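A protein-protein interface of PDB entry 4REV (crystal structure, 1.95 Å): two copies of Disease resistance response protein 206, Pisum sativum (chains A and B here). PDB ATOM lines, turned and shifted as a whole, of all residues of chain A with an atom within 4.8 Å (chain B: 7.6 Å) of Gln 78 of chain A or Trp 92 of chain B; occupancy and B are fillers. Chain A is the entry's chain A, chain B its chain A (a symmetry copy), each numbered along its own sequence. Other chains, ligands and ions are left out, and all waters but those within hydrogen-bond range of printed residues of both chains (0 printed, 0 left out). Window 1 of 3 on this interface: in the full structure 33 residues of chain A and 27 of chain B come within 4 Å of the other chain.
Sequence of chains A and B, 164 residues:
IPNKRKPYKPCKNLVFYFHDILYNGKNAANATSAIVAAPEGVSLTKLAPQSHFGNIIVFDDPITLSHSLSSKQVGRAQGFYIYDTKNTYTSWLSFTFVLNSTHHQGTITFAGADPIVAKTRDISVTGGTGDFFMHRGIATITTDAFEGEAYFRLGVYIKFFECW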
ATOM      1  N   PHE A  59     -12.297 -29.794  14.527  1.00  0.00           N
ATOM      2  CA  PHE A  59     -13.511 -29.114  14.112  1.00  0.00           C
ATOM      3  C   PHE A  59     -13.247 -27.675  13.656  1.00  0.00           C
ATOM      4  O   PHE A  59     -12.268 -27.041  14.050  1.00  0.00           O
ATOM      5  CB  PHE A  59     -14.539 -29.153  15.248  1.00  0.00           C
ATOM      6  CG  PHE A  59     -14.083 -28.470  16.529  1.00  0.00           C
ATOM      7  CD1 PHE A  59     -14.298 -27.117  16.719  1.00  0.00           C
ATOM      8  CD2 PHE A  59     -13.492 -29.197  17.553  1.00  0.00           C
ATOM      9  CE1 PHE A  59     -13.906 -26.484  17.918  1.00  0.00           C
ATOM     10  CE2 PHE A  59     -13.097 -28.578  18.746  1.00  0.00           C
ATOM     11  CZ  PHE A  59     -13.312 -27.222  18.920  1.00  0.00           C
ATOM     12  N   ASP A  60     -14.133 -27.182  12.798  1.00  0.00           N
ATOM     13  CA  ASP A  60     -14.084 -25.817  12.286  1.00  0.00           C
ATOM     14  C   ASP A  60     -15.528 -25.360  12.216  1.00  0.00           C
ATOM     15  O   ASP A  60     -16.250 -25.729  11.300  1.00  0.00           O
ATOM     16  CB  ASP A  60     -13.394 -25.760  10.915  1.00  0.00           C
ATOM     17  CG  ASP A  60     -13.465 -24.375  10.262  1.00  0.00           C
ATOM     18  OD1 ASP A  60     -13.844 -23.383  10.923  1.00  0.00           O
ATOM     19  OD2 ASP A  60     -13.096 -24.273   9.077  1.00  0.00           O
ATOM     20  N   ARG A  76     -14.887 -18.204  13.281  1.00  0.00           N
ATOM     21  CA  ARG A  76     -14.876 -19.658  13.303  1.00  0.00           C
ATOM     22  C   ARG A  76     -14.235 -20.153  14.589  1.00  0.00           C
ATOM     23  O   ARG A  76     -13.223 -19.591  15.058  1.00  0.00           O
ATOM     24  CB  ARG A  76     -14.093 -20.235  12.114  1.00  0.00           C
ATOM     25  CG  ARG A  76     -14.577 -19.811  10.718  1.00  0.00           C
ATOM     26  CD  ARG A  76     -16.014 -20.229  10.415  1.00  0.00           C
ATOM     27  NE  ARG A  76     -16.146 -21.678  10.254  1.00  0.00           N
ATOM     28  CZ  ARG A  76     -17.227 -22.272   9.764  1.00  0.00           C
ATOM     29  NH1 ARG A  76     -18.263 -21.538   9.368  1.00  0.00           N
ATOM     30  NH2 ARG A  76     -17.274 -23.596   9.656  1.00  0.00           N
ATOM     31  N   ALA A  77     -14.813 -21.205  15.153  1.00  0.00           N
ATOM     32  CA  ALA A  77     -14.198 -21.901  16.288  1.00  0.00           C
ATOM     33  C   ALA A  77     -13.394 -23.057  15.720  1.00  0.00           C
ATOM     34  O   ALA A  77     -13.943 -23.946  15.077  1.00  0.00           O
ATOM     35  CB  ALA A  77     -15.254 -22.407  17.283  1.00  0.00           C
ATOM     36  N   GLN A  78     -12.084 -23.039  15.934  1.00  0.00           N
ATOM     37  CA  GLN A  78     -11.242 -24.067  15.330  1.00  0.00           C
ATOM     38  C   GLN A  78     -10.360 -24.677  16.397  1.00  0.00           C
ATOM     39  O   GLN A  78      -9.665 -23.963  17.124  1.00  0.00           O
ATOM     40  CB  GLN A  78     -10.407 -23.478  14.191  1.00  0.00           C
ATOM     41  CG  GLN A  78     -11.251 -22.653  13.197  1.00  0.00           C
ATOM     42  CD  GLN A  78     -10.447 -22.148  12.020  1.00  0.00           C
ATOM     43  OE1 GLN A  78      -9.241 -21.950  12.124  1.00  0.00           O
ATOM     44  NE2 GLN A  78     -11.113 -21.933  10.891  1.00  0.00           N
ATOM     45  N   GLY A  79     -10.425 -25.996  16.527  1.00  0.00           N
ATOM     46  CA  GLY A  79      -9.594 -26.679  17.505  1.00  0.00           C
ATOM     47  C   GLY A  79      -9.745 -28.178  17.418  1.00  0.00           C
ATOM     48  O   GLY A  79     -10.037 -28.728  16.334  1.00  0.00           O
ATOM     49  N   PHE A  80      -9.557 -28.851  18.546  1.00  0.00           N
ATOM     50  CA  PHE A  80      -9.685 -30.304  18.526  1.00  0.00           C
ATOM     51  C   PHE A  80     -10.137 -30.822  19.878  1.00  0.00           C
ATOM     52  O   PHE A  80     -10.045 -30.131  20.894  1.00  0.00           O
ATOM     53  CB  PHE A  80      -8.357 -30.971  18.111  1.00  0.00           C
ATOM     54  CG  PHE A  80      -7.248 -30.847  19.145  1.00  0.00           C
ATOM     55  CD1 PHE A  80      -6.395 -29.751  19.138  1.00  0.00           C
ATOM     56  CD2 PHE A  80      -7.068 -31.827  20.114  1.00  0.00           C
ATOM     57  CE1 PHE A  80      -5.372 -29.632  20.082  1.00  0.00           C
ATOM     58  CE2 PHE A  80      -6.060 -31.715  21.063  1.00  0.00           C
ATOM     59  CZ  PHE A  80      -5.207 -30.612  21.047  1.00  0.00           C
ATOM     60  N   SER A  94      -9.094 -28.175  23.231  1.00  0.00           N
ATOM     61  CA  SER A  94      -8.245 -27.045  22.875  1.00  0.00           C
ATOM     62  C   SER A  94      -8.870 -26.362  21.690  1.00  0.00           C
ATOM     63  O   SER A  94      -9.113 -27.002  20.676  1.00  0.00           O
ATOM     64  CB  SER A  94      -6.821 -27.480  22.506  1.00  0.00           C
ATOM     65  OG  SER A  94      -6.193 -28.180  23.547  1.00  0.00           O
ATOM     66  N   PHE A  95      -9.154 -25.073  21.797  1.00  0.00           N
ATOM     67  CA  PHE A  95      -9.676 -24.385  20.633  1.00  0.00           C
ATOM     68  C   PHE A  95      -9.457 -22.883  20.677  1.00  0.00           C
ATOM     69  O   PHE A  95      -9.167 -22.307  21.717  1.00  0.00           O
ATOM     70  CB  PHE A  95     -11.168 -24.690  20.435  1.00  0.00           C
ATOM     71  CG  PHE A  95     -12.066 -24.153  21.523  1.00  0.00           C
ATOM     72  CD1 PHE A  95     -12.262 -24.867  22.694  1.00  0.00           C
ATOM     73  CD2 PHE A  95     -12.757 -22.957  21.349  1.00  0.00           C
ATOM     74  CE1 PHE A  95     -13.112 -24.387  23.697  1.00  0.00           C
ATOM     75  CE2 PHE A  95     -13.613 -22.466  22.346  1.00  0.00           C
ATOM     76  CZ  PHE A  95     -13.784 -23.189  23.523  1.00  0.00           C
ATOM     77  N   THR A  96      -9.596 -22.282  19.502  1.00  0.00           N
ATOM     78  CA  THR A  96      -9.370 -20.863  19.278  1.00  0.00           C
ATOM     79  C   THR A  96     -10.623 -20.279  18.622  1.00  0.00           C
ATOM     80  O   THR A  96     -11.134 -20.830  17.650  1.00  0.00           O
ATOM     81  CB  THR A  96      -8.151 -20.633  18.353  1.00  0.00           C
ATOM     82  OG1 THR A  96      -6.967 -21.165  18.974  1.00  0.00           O
ATOM     83  CG2 THR A  96      -7.979 -19.133  18.037  1.00  0.00           C
ATOM     84  N   VAL A  98     -11.533 -17.689  16.246  1.00  0.00           N
ATOM     85  CA  VAL A  98     -10.926 -16.813  15.261  1.00  0.00           C
ATOM     86  C   VAL A  98     -11.970 -15.793  14.848  1.00  0.00           C
ATOM     87  O   VAL A  98     -12.834 -16.082  14.027  1.00  0.00           O
ATOM     88  CB  VAL A  98     -10.420 -17.584  14.035  1.00  0.00           C
ATOM     89  CG1 VAL A  98      -9.807 -16.621  12.999  1.00  0.00           C
ATOM     90  CG2 VAL A  98      -9.408 -18.635  14.465  1.00  0.00           C
ATOM     91  N   THR A 109      -7.848 -18.135  22.602  1.00  0.00           N
ATOM     92  CA  THR A 109      -7.566 -19.560  22.692  1.00  0.00           C
ATOM     93  C   THR A 109      -7.875 -20.070  24.101  1.00  0.00           C
ATOM     94  O   THR A 109      -7.634 -19.377  25.114  1.00  0.00           O
ATOM     95  CB  THR A 109      -6.096 -19.829  22.285  1.00  0.00           C
ATOM     96  OG1 THR A 109      -5.925 -19.446  20.905  1.00  0.00           O
ATOM     97  CG2 THR A 109      -5.686 -21.317  22.470  1.00  0.00           C
ATOM     98  N   LYS B  46     -22.276 -19.103   6.510  1.00  0.00           N
ATOM     99  CA  LYS B  46     -21.227 -19.378   5.523  1.00  0.00           C
ATOM    100  C   LYS B  46     -21.106 -20.920   5.536  1.00  0.00           C
ATOM    101  O   LYS B  46     -22.112 -21.613   5.419  1.00  0.00           O
ATOM    102  CB  LYS B  46     -19.913 -18.567   5.842  1.00  0.00           C
ATOM    103  CG  LYS B  46     -18.502 -19.122   5.447  1.00  0.00           C
ATOM    104  CD  LYS B  46     -17.245 -18.372   5.932  1.00  0.00           C
ATOM    105  CE  LYS B  46     -16.821 -18.688   7.345  1.00  0.00           C
ATOM    106  NZ  LYS B  46     -15.761 -17.766   7.875  1.00  0.00           N
ATOM    107  N   LEU B  47     -19.903 -21.442   5.702  1.00  0.00           N
ATOM    108  CA  LEU B  47     -19.612 -22.854   5.819  1.00  0.00           C
ATOM    109  C   LEU B  47     -20.321 -23.457   7.030  1.00  0.00           C
ATOM    110  O   LEU B  47     -20.350 -22.858   8.101  1.00  0.00           O
ATOM    111  CB  LEU B  47     -18.095 -23.031   5.918  1.00  0.00           C
ATOM    112  CG  LEU B  47     -17.406 -24.329   5.499  1.00  0.00           C
ATOM    113  CD1 LEU B  47     -17.564 -24.602   4.000  1.00  0.00           C
ATOM    114  CD2 LEU B  47     -15.933 -24.225   5.879  1.00  0.00           C
ATOM    115  N   GLN B  50     -17.932 -28.165  10.748  1.00  0.00           N
ATOM    116  CA  GLN B  50     -17.248 -29.077   9.907  1.00  0.00           C
ATOM    117  C   GLN B  50     -16.418 -29.858  10.956  1.00  0.00           C
ATOM    118  O   GLN B  50     -15.788 -29.243  11.790  1.00  0.00           O
ATOM    119  CB  GLN B  50     -16.347 -28.364   8.918  1.00  0.00           C
ATOM    120  CG  GLN B  50     -16.806 -28.311   7.450  1.00  0.00           C
ATOM    121  CD  GLN B  50     -15.617 -27.837   6.612  1.00  0.00           C
ATOM    122  OE1 GLN B  50     -15.244 -28.583   5.674  1.00  0.00           O
ATOM    123  NE2 GLN B  50     -14.811 -26.861   7.169  1.00  0.00           N
ATOM    124  N   PHE B  59       6.923 -32.631  15.401  1.00  0.00           N
ATOM    125  CA  PHE B  59       8.177 -32.159  14.846  1.00  0.00           C
ATOM    126  C   PHE B  59       9.186 -31.770  15.933  1.00  0.00           C
ATOM    127  O   PHE B  59       8.824 -31.433  17.061  1.00  0.00           O
ATOM    128  CB  PHE B  59       7.914 -30.987  13.895  1.00  0.00           C
ATOM    129  CG  PHE B  59       7.256 -29.782  14.552  1.00  0.00           C
ATOM    130  CD1 PHE B  59       8.025 -28.797  15.146  1.00  0.00           C
ATOM    131  CD2 PHE B  59       5.878 -29.617  14.524  1.00  0.00           C
ATOM    132  CE1 PHE B  59       7.423 -27.662  15.729  1.00  0.00           C
ATOM    133  CE2 PHE B  59       5.271 -28.496  15.102  1.00  0.00           C
ATOM    134  CZ  PHE B  59       6.052 -27.522  15.699  1.00  0.00           C
ATOM    135  N   PHE B  80       3.525 -29.964  17.830  1.00  0.00           N
ATOM    136  CA  PHE B  80       2.752 -30.764  16.887  1.00  0.00           C
ATOM    137  C   PHE B  80       1.787 -29.892  16.105  1.00  0.00           C
ATOM    138  O   PHE B  80       1.484 -28.763  16.495  1.00  0.00           O
ATOM    139  CB  PHE B  80       1.990 -31.893  17.610  1.00  0.00           C
ATOM    140  CG  PHE B  80       0.851 -31.408  18.495  1.00  0.00           C
ATOM    141  CD1 PHE B  80       1.081 -31.069  19.822  1.00  0.00           C
ATOM    142  CD2 PHE B  80      -0.440 -31.294  17.991  1.00  0.00           C
ATOM    143  CE1 PHE B  80       0.040 -30.625  20.640  1.00  0.00           C
ATOM    144  CE2 PHE B  80      -1.482 -30.845  18.793  1.00  0.00           C
ATOM    145  CZ  PHE B  80      -1.241 -30.510  20.125  1.00  0.00           C
ATOM    146  N   TYR B  81       1.336 -30.416  14.974  1.00  0.00           N
ATOM    147  CA  TYR B  81       0.192 -29.854  14.289  1.00  0.00           C
ATOM    148  C   TYR B  81      -0.624 -30.992  13.705  1.00  0.00           C
ATOM    149  O   TYR B  81      -0.285 -32.170  13.864  1.00  0.00           O
ATOM    150  CB  TYR B  81       0.609 -28.867  13.197  1.00  0.00           C
ATOM    151  CG  TYR B  81       1.407 -29.471  12.075  1.00  0.00           C
ATOM    152  CD1 TYR B  81       2.781 -29.644  12.186  1.00  0.00           C
ATOM    153  CD2 TYR B  81       0.787 -29.861  10.890  1.00  0.00           C
ATOM    154  CE1 TYR B  81       3.517 -30.204  11.144  1.00  0.00           C
ATOM    155  CE2 TYR B  81       1.512 -30.415   9.848  1.00  0.00           C
ATOM    156  CZ  TYR B  81       2.875 -30.583   9.983  1.00  0.00           C
ATOM    157  OH  TYR B  81       3.597 -31.134   8.953  1.00  0.00           O
ATOM    158  N   ILE B  82      -1.692 -30.630  13.013  1.00  0.00           N
ATOM    159  CA  ILE B  82      -2.698 -31.590  12.607  1.00  0.00           C
ATOM    160  C   ILE B  82      -2.911 -31.579  11.103  1.00  0.00           C
ATOM    161  O   ILE B  82      -2.907 -30.523  10.488  1.00  0.00           O
ATOM    162  CB  ILE B  82      -4.036 -31.286  13.299  1.00  0.00           C
ATOM    163  CG1 ILE B  82      -3.888 -31.431  14.812  1.00  0.00           C
ATOM    164  CG2 ILE B  82      -5.116 -32.209  12.797  1.00  0.00           C
ATOM    165  CD1 ILE B  82      -5.049 -30.874  15.582  1.00  0.00           C
ATOM    166  N   TYR B  83      -3.073 -32.751  10.501  1.00  0.00           N
ATOM    167  CA  TYR B  83      -3.662 -32.803   9.172  1.00  0.00           C
ATOM    168  C   TYR B  83      -5.097 -33.309   9.272  1.00  0.00           C
ATOM    169  O   TYR B  83      -5.407 -34.147  10.108  1.00  0.00           O
ATOM    170  CB  TYR B  83      -2.838 -33.678   8.224  1.00  0.00           C
ATOM    171  CG  TYR B  83      -1.795 -32.889   7.472  1.00  0.00           C
ATOM    172  CD1 TYR B  83      -1.889 -31.505   7.392  1.00  0.00           C
ATOM    173  CD2 TYR B  83      -0.732 -33.514   6.827  1.00  0.00           C
ATOM    174  CE1 TYR B  83      -0.952 -30.761   6.707  1.00  0.00           C
ATOM    175  CE2 TYR B  83       0.219 -32.771   6.133  1.00  0.00           C
ATOM    176  CZ  TYR B  83       0.099 -31.394   6.080  1.00  0.00           C
ATOM    177  OH  TYR B  83       1.027 -30.637   5.401  1.00  0.00           O
ATOM    178  N   THR B  90      -7.054 -27.487  10.384  1.00  0.00           N
ATOM    179  CA  THR B  90      -5.634 -27.711  10.631  1.00  0.00           C
ATOM    180  C   THR B  90      -4.849 -26.422  10.651  1.00  0.00           C
ATOM    181  O   THR B  90      -3.685 -26.375  10.254  1.00  0.00           O
ATOM    182  CB  THR B  90      -5.034 -28.627   9.587  1.00  0.00           C
ATOM    183  OG1 THR B  90      -4.912 -27.934   8.338  1.00  0.00           O
ATOM    184  CG2 THR B  90      -5.913 -29.830   9.422  1.00  0.00           C
ATOM    185  N   SER B  91      -5.495 -25.368  11.117  1.00  0.00           N
ATOM    186  CA  SER B  91      -4.773 -24.153  11.424  1.00  0.00           C
ATOM    187  C   SER B  91      -4.164 -24.301  12.807  1.00  0.00           C
ATOM    188  O   SER B  91      -3.494 -23.383  13.285  1.00  0.00           O
ATOM    189  CB  SER B  91      -5.687 -22.927  11.355  1.00  0.00           C
ATOM    190  OG  SER B  91      -6.966 -23.202  11.904  1.00  0.00           O
ATOM    191  N   TRP B  92      -4.379 -25.460  13.442  1.00  0.00           N
ATOM    192  CA  TRP B  92      -3.937 -25.649  14.829  1.00  0.00           C
ATOM    193  C   TRP B  92      -2.452 -25.960  14.998  1.00  0.00           C
ATOM    194  O   TRP B  92      -1.901 -26.864  14.358  1.00  0.00           O
ATOM    195  CB  TRP B  92      -4.720 -26.762  15.537  1.00  0.00           C
ATOM    196  CG  TRP B  92      -4.332 -26.747  16.973  1.00  0.00           C
ATOM    197  CD1 TRP B  92      -3.301 -27.430  17.558  1.00  0.00           C
ATOM    198  CD2 TRP B  92      -4.895 -25.920  18.000  1.00  0.00           C
ATOM    199  NE1 TRP B  92      -3.204 -27.098  18.890  1.00  0.00           N
ATOM    200  CE2 TRP B  92      -4.182 -26.183  19.189  1.00  0.00           C
ATOM    201  CE3 TRP B  92      -5.951 -25.005  18.034  1.00  0.00           C
ATOM    202  CZ2 TRP B  92      -4.481 -25.549  20.401  1.00  0.00           C
ATOM    203  CZ3 TRP B  92      -6.250 -24.375  19.243  1.00  0.00           C
ATOM    204  CH2 TRP B  92      -5.520 -24.655  20.404  1.00  0.00           C
ATOM    205  N   LEU B  93      -1.830 -25.245  15.930  1.00  0.00           N
ATOM    206  CA  LEU B  93      -0.410 -25.365  16.161  1.00  0.00           C
ATOM    207  C   LEU B  93      -0.150 -25.276  17.662  1.00  0.00           C
ATOM    208  O   LEU B  93      -0.714 -24.427  18.319  1.00  0.00           O
ATOM    209  CB  LEU B  93       0.310 -24.254  15.398  1.00  0.00           C
ATOM    210  CG  LEU B  93       1.819 -24.127  15.302  1.00  0.00           C
ATOM    211  CD1 LEU B  93       2.479 -25.477  15.041  1.00  0.00           C
ATOM    212  CD2 LEU B  93       2.108 -23.159  14.164  1.00  0.00           C
ATOM    213  N   SER B  94       0.641 -26.200  18.202  1.00  0.00           N
ATOM    214  CA  SER B  94       1.121 -26.104  19.575  1.00  0.00           C
ATOM    215  C   SER B  94       2.596 -26.403  19.564  1.00  0.00           C
ATOM    216  O   SER B  94       3.001 -27.453  19.081  1.00  0.00           O
ATOM    217  CB  SER B  94       0.417 -27.097  20.508  1.00  0.00           C
ATOM    218  OG  SER B  94      -0.974 -26.917  20.523  1.00  0.00           O
ATOM    219  N   PHE B  95       3.415 -25.496  20.071  1.00  0.00           N
ATOM    220  CA  PHE B  95       4.828 -25.810  20.145  1.00  0.00           C
ATOM    221  C   PHE B  95       5.569 -24.994  21.189  1.00  0.00           C
ATOM    222  O   PHE B  95       5.087 -23.978  21.671  1.00  0.00           O
ATOM    223  CB  PHE B  95       5.502 -25.643  18.776  1.00  0.00           C
ATOM    224  CG  PHE B  95       5.541 -24.223  18.267  1.00  0.00           C
ATOM    225  CD1 PHE B  95       4.457 -23.682  17.595  1.00  0.00           C
ATOM    226  CD2 PHE B  95       6.689 -23.446  18.415  1.00  0.00           C
ATOM    227  CE1 PHE B  95       4.496 -22.373  17.100  1.00  0.00           C
ATOM    228  CE2 PHE B  95       6.739 -22.134  17.921  1.00  0.00           C
ATOM    229  CZ  PHE B  95       5.633 -21.602  17.264  1.00  0.00           C
ATOM    230  N   PHE B 110       3.729 -21.795  22.665  1.00  0.00           N
ATOM    231  CA  PHE B 110       2.739 -21.064  21.878  1.00  0.00           C
ATOM    232  C   PHE B 110       1.618 -22.019  21.505  1.00  0.00           C
ATOM    233  O   PHE B 110       1.885 -23.191  21.237  1.00  0.00           O
ATOM    234  CB  PHE B 110       3.347 -20.489  20.583  1.00  0.00           C
ATOM    235  CG  PHE B 110       4.667 -19.788  20.758  1.00  0.00           C
ATOM    236  CD1 PHE B 110       5.856 -20.498  20.765  1.00  0.00           C
ATOM    237  CD2 PHE B 110       4.713 -18.397  20.873  1.00  0.00           C
ATOM    238  CE1 PHE B 110       7.079 -19.845  20.895  1.00  0.00           C
ATOM    239  CE2 PHE B 110       5.935 -17.735  21.005  1.00  0.00           C
ATOM    240  CZ  PHE B 110       7.115 -18.467  21.018  1.00  0.00           C
ATOM    241  N   ALA B 111       0.388 -21.531  21.421  1.00  0.00           N
ATOM    242  CA  ALA B 111      -0.719 -22.420  21.010  1.00  0.00           C
ATOM    243  C   ALA B 111      -1.837 -21.631  20.347  1.00  0.00           C
ATOM    244  O   ALA B 111      -2.093 -20.489  20.725  1.00  0.00           O
ATOM    245  CB  ALA B 111      -1.274 -23.201  22.221  1.00  0.00           C
ATOM    246  N   GLY B 112      -2.502 -22.236  19.363  1.00  0.00           N
ATOM    247  CA  GLY B 112      -3.655 -21.583  18.778  1.00  0.00           C
ATOM    248  C   GLY B 112      -3.838 -21.916  17.313  1.00  0.00           C
ATOM    249  O   GLY B 112      -2.997 -22.569  16.695  1.00  0.00           O
ATOM    250  N   ALA B 113      -4.968 -21.486  16.768  1.00  0.00           N
ATOM    251  CA  ALA B 113      -5.221 -21.596  15.335  1.00  0.00           C
ATOM    252  C   ALA B 113      -5.300 -20.203  14.723  1.00  0.00           C
ATOM    253  O   ALA B 113      -5.836 -19.288  15.338  1.00  0.00           O
ATOM    254  CB  ALA B 113      -6.503 -22.372  15.074  1.00  0.00           C
ATOM    255  N   ASP B 114      -4.723 -20.047  13.534  1.00  0.00           N
ATOM    256  CA  ASP B 114      -4.819 -18.826  12.726  1.00  0.00           C
ATOM    257  C   ASP B 114      -4.651 -19.290  11.278  1.00  0.00           C
ATOM    258  O   ASP B 114      -3.626 -19.889  10.949  1.00  0.00           O
ATOM    259  CB  ASP B 114      -3.752 -17.791  13.132  1.00  0.00           C
ATOM    260  CG  ASP B 114      -4.188 -16.344  12.876  1.00  0.00           C
ATOM    261  OD1 ASP B 114      -5.407 -16.066  12.816  1.00  0.00           O
ATOM    262  OD2 ASP B 114      -3.299 -15.474  12.744  1.00  0.00           O
ATOM    263  N   PRO B 115      -5.642 -19.002  10.414  1.00  0.00           N
ATOM    264  CA  PRO B 115      -5.913 -19.765   9.183  1.00  0.00           C
ATOM    265  C   PRO B 115      -4.687 -20.060   8.321  1.00  0.00           C
ATOM    266  O   PRO B 115      -4.336 -21.235   8.200  1.00  0.00           O
ATOM    267  CB  PRO B 115      -6.893 -18.859   8.428  1.00  0.00           C
ATOM    268  CG  PRO B 115      -6.547 -17.494   8.887  1.00  0.00           C
ATOM    269  CD  PRO B 115      -6.270 -17.671  10.356  1.00  0.00           C
ATOM    270  N   ARG B 121       1.328 -14.976  10.228  1.00  0.00           N
ATOM    271  CA  ARG B 121       0.255 -15.052  11.222  1.00  0.00           C
ATOM    272  C   ARG B 121       0.788 -14.711  12.614  1.00  0.00           C
ATOM    273  O   ARG B 121       1.998 -14.788  12.856  1.00  0.00           O
ATOM    274  CB  ARG B 121      -0.392 -16.450  11.233  1.00  0.00           C
ATOM    275  CG  ARG B 121       0.607 -17.613  11.250  1.00  0.00           C
ATOM    276  CD  ARG B 121      -0.069 -18.957  11.525  1.00  0.00           C
ATOM    277  NE  ARG B 121      -0.517 -19.077  12.913  1.00  0.00           N
ATOM    278  CZ  ARG B 121      -1.286 -20.063  13.369  1.00  0.00           C
ATOM    279  NH1 ARG B 121      -1.711 -21.013  12.541  1.00  0.00           N
ATOM    280  NH2 ARG B 121      -1.652 -20.090  14.650  1.00  0.00           N
ATOM    281  N   ILE B 123       0.582 -15.620  16.823  1.00  0.00           N
ATOM    282  CA  ILE B 123       0.192 -16.684  17.745  1.00  0.00           C
ATOM    283  C   ILE B 123       0.503 -16.224  19.168  1.00  0.00           C
ATOM    284  O   ILE B 123       1.477 -15.509  19.392  1.00  0.00           O
ATOM    285  CB  ILE B 123       0.900 -18.036  17.399  1.00  0.00           C
ATOM    286  CG1 ILE B 123       0.239 -19.223  18.114  1.00  0.00           C
ATOM    287  CG2 ILE B 123       2.414 -17.985  17.695  1.00  0.00           C
ATOM    288  CD1 ILE B 123       0.796 -20.598  17.644  1.00  0.00           C
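The side-chain amide oxygen (OE1) of Gln 78 of chain A lies within hydrogen-bond range of the side-chain hydroxyl (OG) of Ser 91 of chain B (2.6 Å).
The guanidinium group (NH1) of Arg 76 of chain A sits at hydrogen-bond distance from the backbone carbonyl oxygen (O) of Leu 47 of chain B.
The backbone carbonyl oxygen of Gln 50 of chain B sits at hydrogen-bond distance from the backbone NH of Asp 60 of chain A, 2.8 Å away.
The side-chain hydroxyl (OG1) of Thr 96 of chain A lies within hydrogen-bond range of the backbone NH (N) of Ala 113 of chain B, 3.0 Å away.
The side-chain amide nitrogen (NE2) of Gln 78 of chain A sits at hydrogen-bond distance from the side-chain carboxylate (OD1) of Asp 60 of chain A, 3.1 Å away.
O of Arg 76 of chain A is in hydrogen-bond range of N of Val 98 of chain A (2.8 Å).
OD1 of Asp 60 of chain A lies within salt-bridge range of NE of Arg 76 of chain A (2.9 Å).
The backbone NH (N) of Phe 80 of chain A is in hydrogen-bond range of the backbone carbonyl oxygen (O) of Ser 94 of chain A (2.9 Å).
The backbone NH of Phe 59 of chain A lies within hydrogen-bond range of the backbone carbonyl oxygen of Gly 79 of chain A, 3.1 Å away.
O of Leu 93 of chain B sits at hydrogen-bond distance from N of Gly 112 of chain B, at 3.0 Å.
Phe 59 of chain A touches Gln 50 of chain B (CA to O, 3.3 Å).
CE of Lys 46 of chain B touches CD of Arg 76 of chain A (3.5 Å).
O of Gln 78 of chain A touches CE3 of Trp 92 of chain B (3.96 Å).
Phe 80 of chain A touches Ile 82 of chain B (CD1 to CD1, 3.96 Å).
Trp 92 of chain B touches Phe 80 of chain A (NE1 to CE1, 3.5 Å).
CZ2 of Trp 92 of chain B touches CB of Ser 94 of chain A, 3.7 Å away.
CA of Phe 95 of chain A touches CZ3 of Trp 92 of chain B, 3.7 Å away.
Thr 96 of chain A touches Trp 92 of chain B.
O of Ala 111 of chain B touches OG1 of Thr 109 of chain A, at 3.98 Å.
Thr 109 of chain A touches Gly 112 of chain B (OG1 to CA, 3.8 Å).
Of chain B, only Ser 91 (2.6 Å) and Trp 92 (3.96 Å) come within 4 Å of Gln 78 of chain A.
Of chain A, only Gln 78, Phe 80, Ser 94, Phe 95, Thr 96 and Thr 109 come within 4 Å of Trp 92 of chain B.
No residue of chain B comes within 4 Å of Ala 77 of chain A.
Of the printed residues of chain A, Gly 112 of chain B touches Thr 96 (3.3 Å) and Thr 109 (3.8 Å).
Printed residues of chain A within 4 Å of Leu 47 of chain B: Arg 76.
Printed residues of chain B within 4 Å of Thr 96 of chain A: Trp 92 (3.3 Å), Gly 112 (3.3 Å) and Ala 113 (3.0 Å).
Printed residues of chain A within 4 Å of Ala 113 of chain B: Thr 96 and Val 98.
Of the printed residues of chain B, Val 98 of chain A touches Ala 113.
Arg 121 of chain B touches none of the printed residues of chain A.
Phe 80 of chain B touches none of the printed residues of chain A.
The nearest residue of chain B that does not touch Gln 78 of chain A is Ala 113 of chain B (4.05 Å).
Of the 22 printed residues of chain B, 9 touch a printed residue of chain A.
Hydrophobic or aromatic side chains of chain B that line the printed part of chain A: Leu 47, Ile 82 and Trp 92.
Along chain B the printed residues that touch a printed residue of chain A span positions 46 to 113.
Hydrophobic or aromatic side chains of chain A within 4 Å of the printed part of chain B: Phe 59, Phe 80 and Val 98.
Among the printed residues, 17 pairs touch across the chains.
Among the printed residues, no Asp or Glu carboxylate lies within 4 Å of a Lys or Arg side-chain nitrogen of the other chain.
4 positions are printed for both chains.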
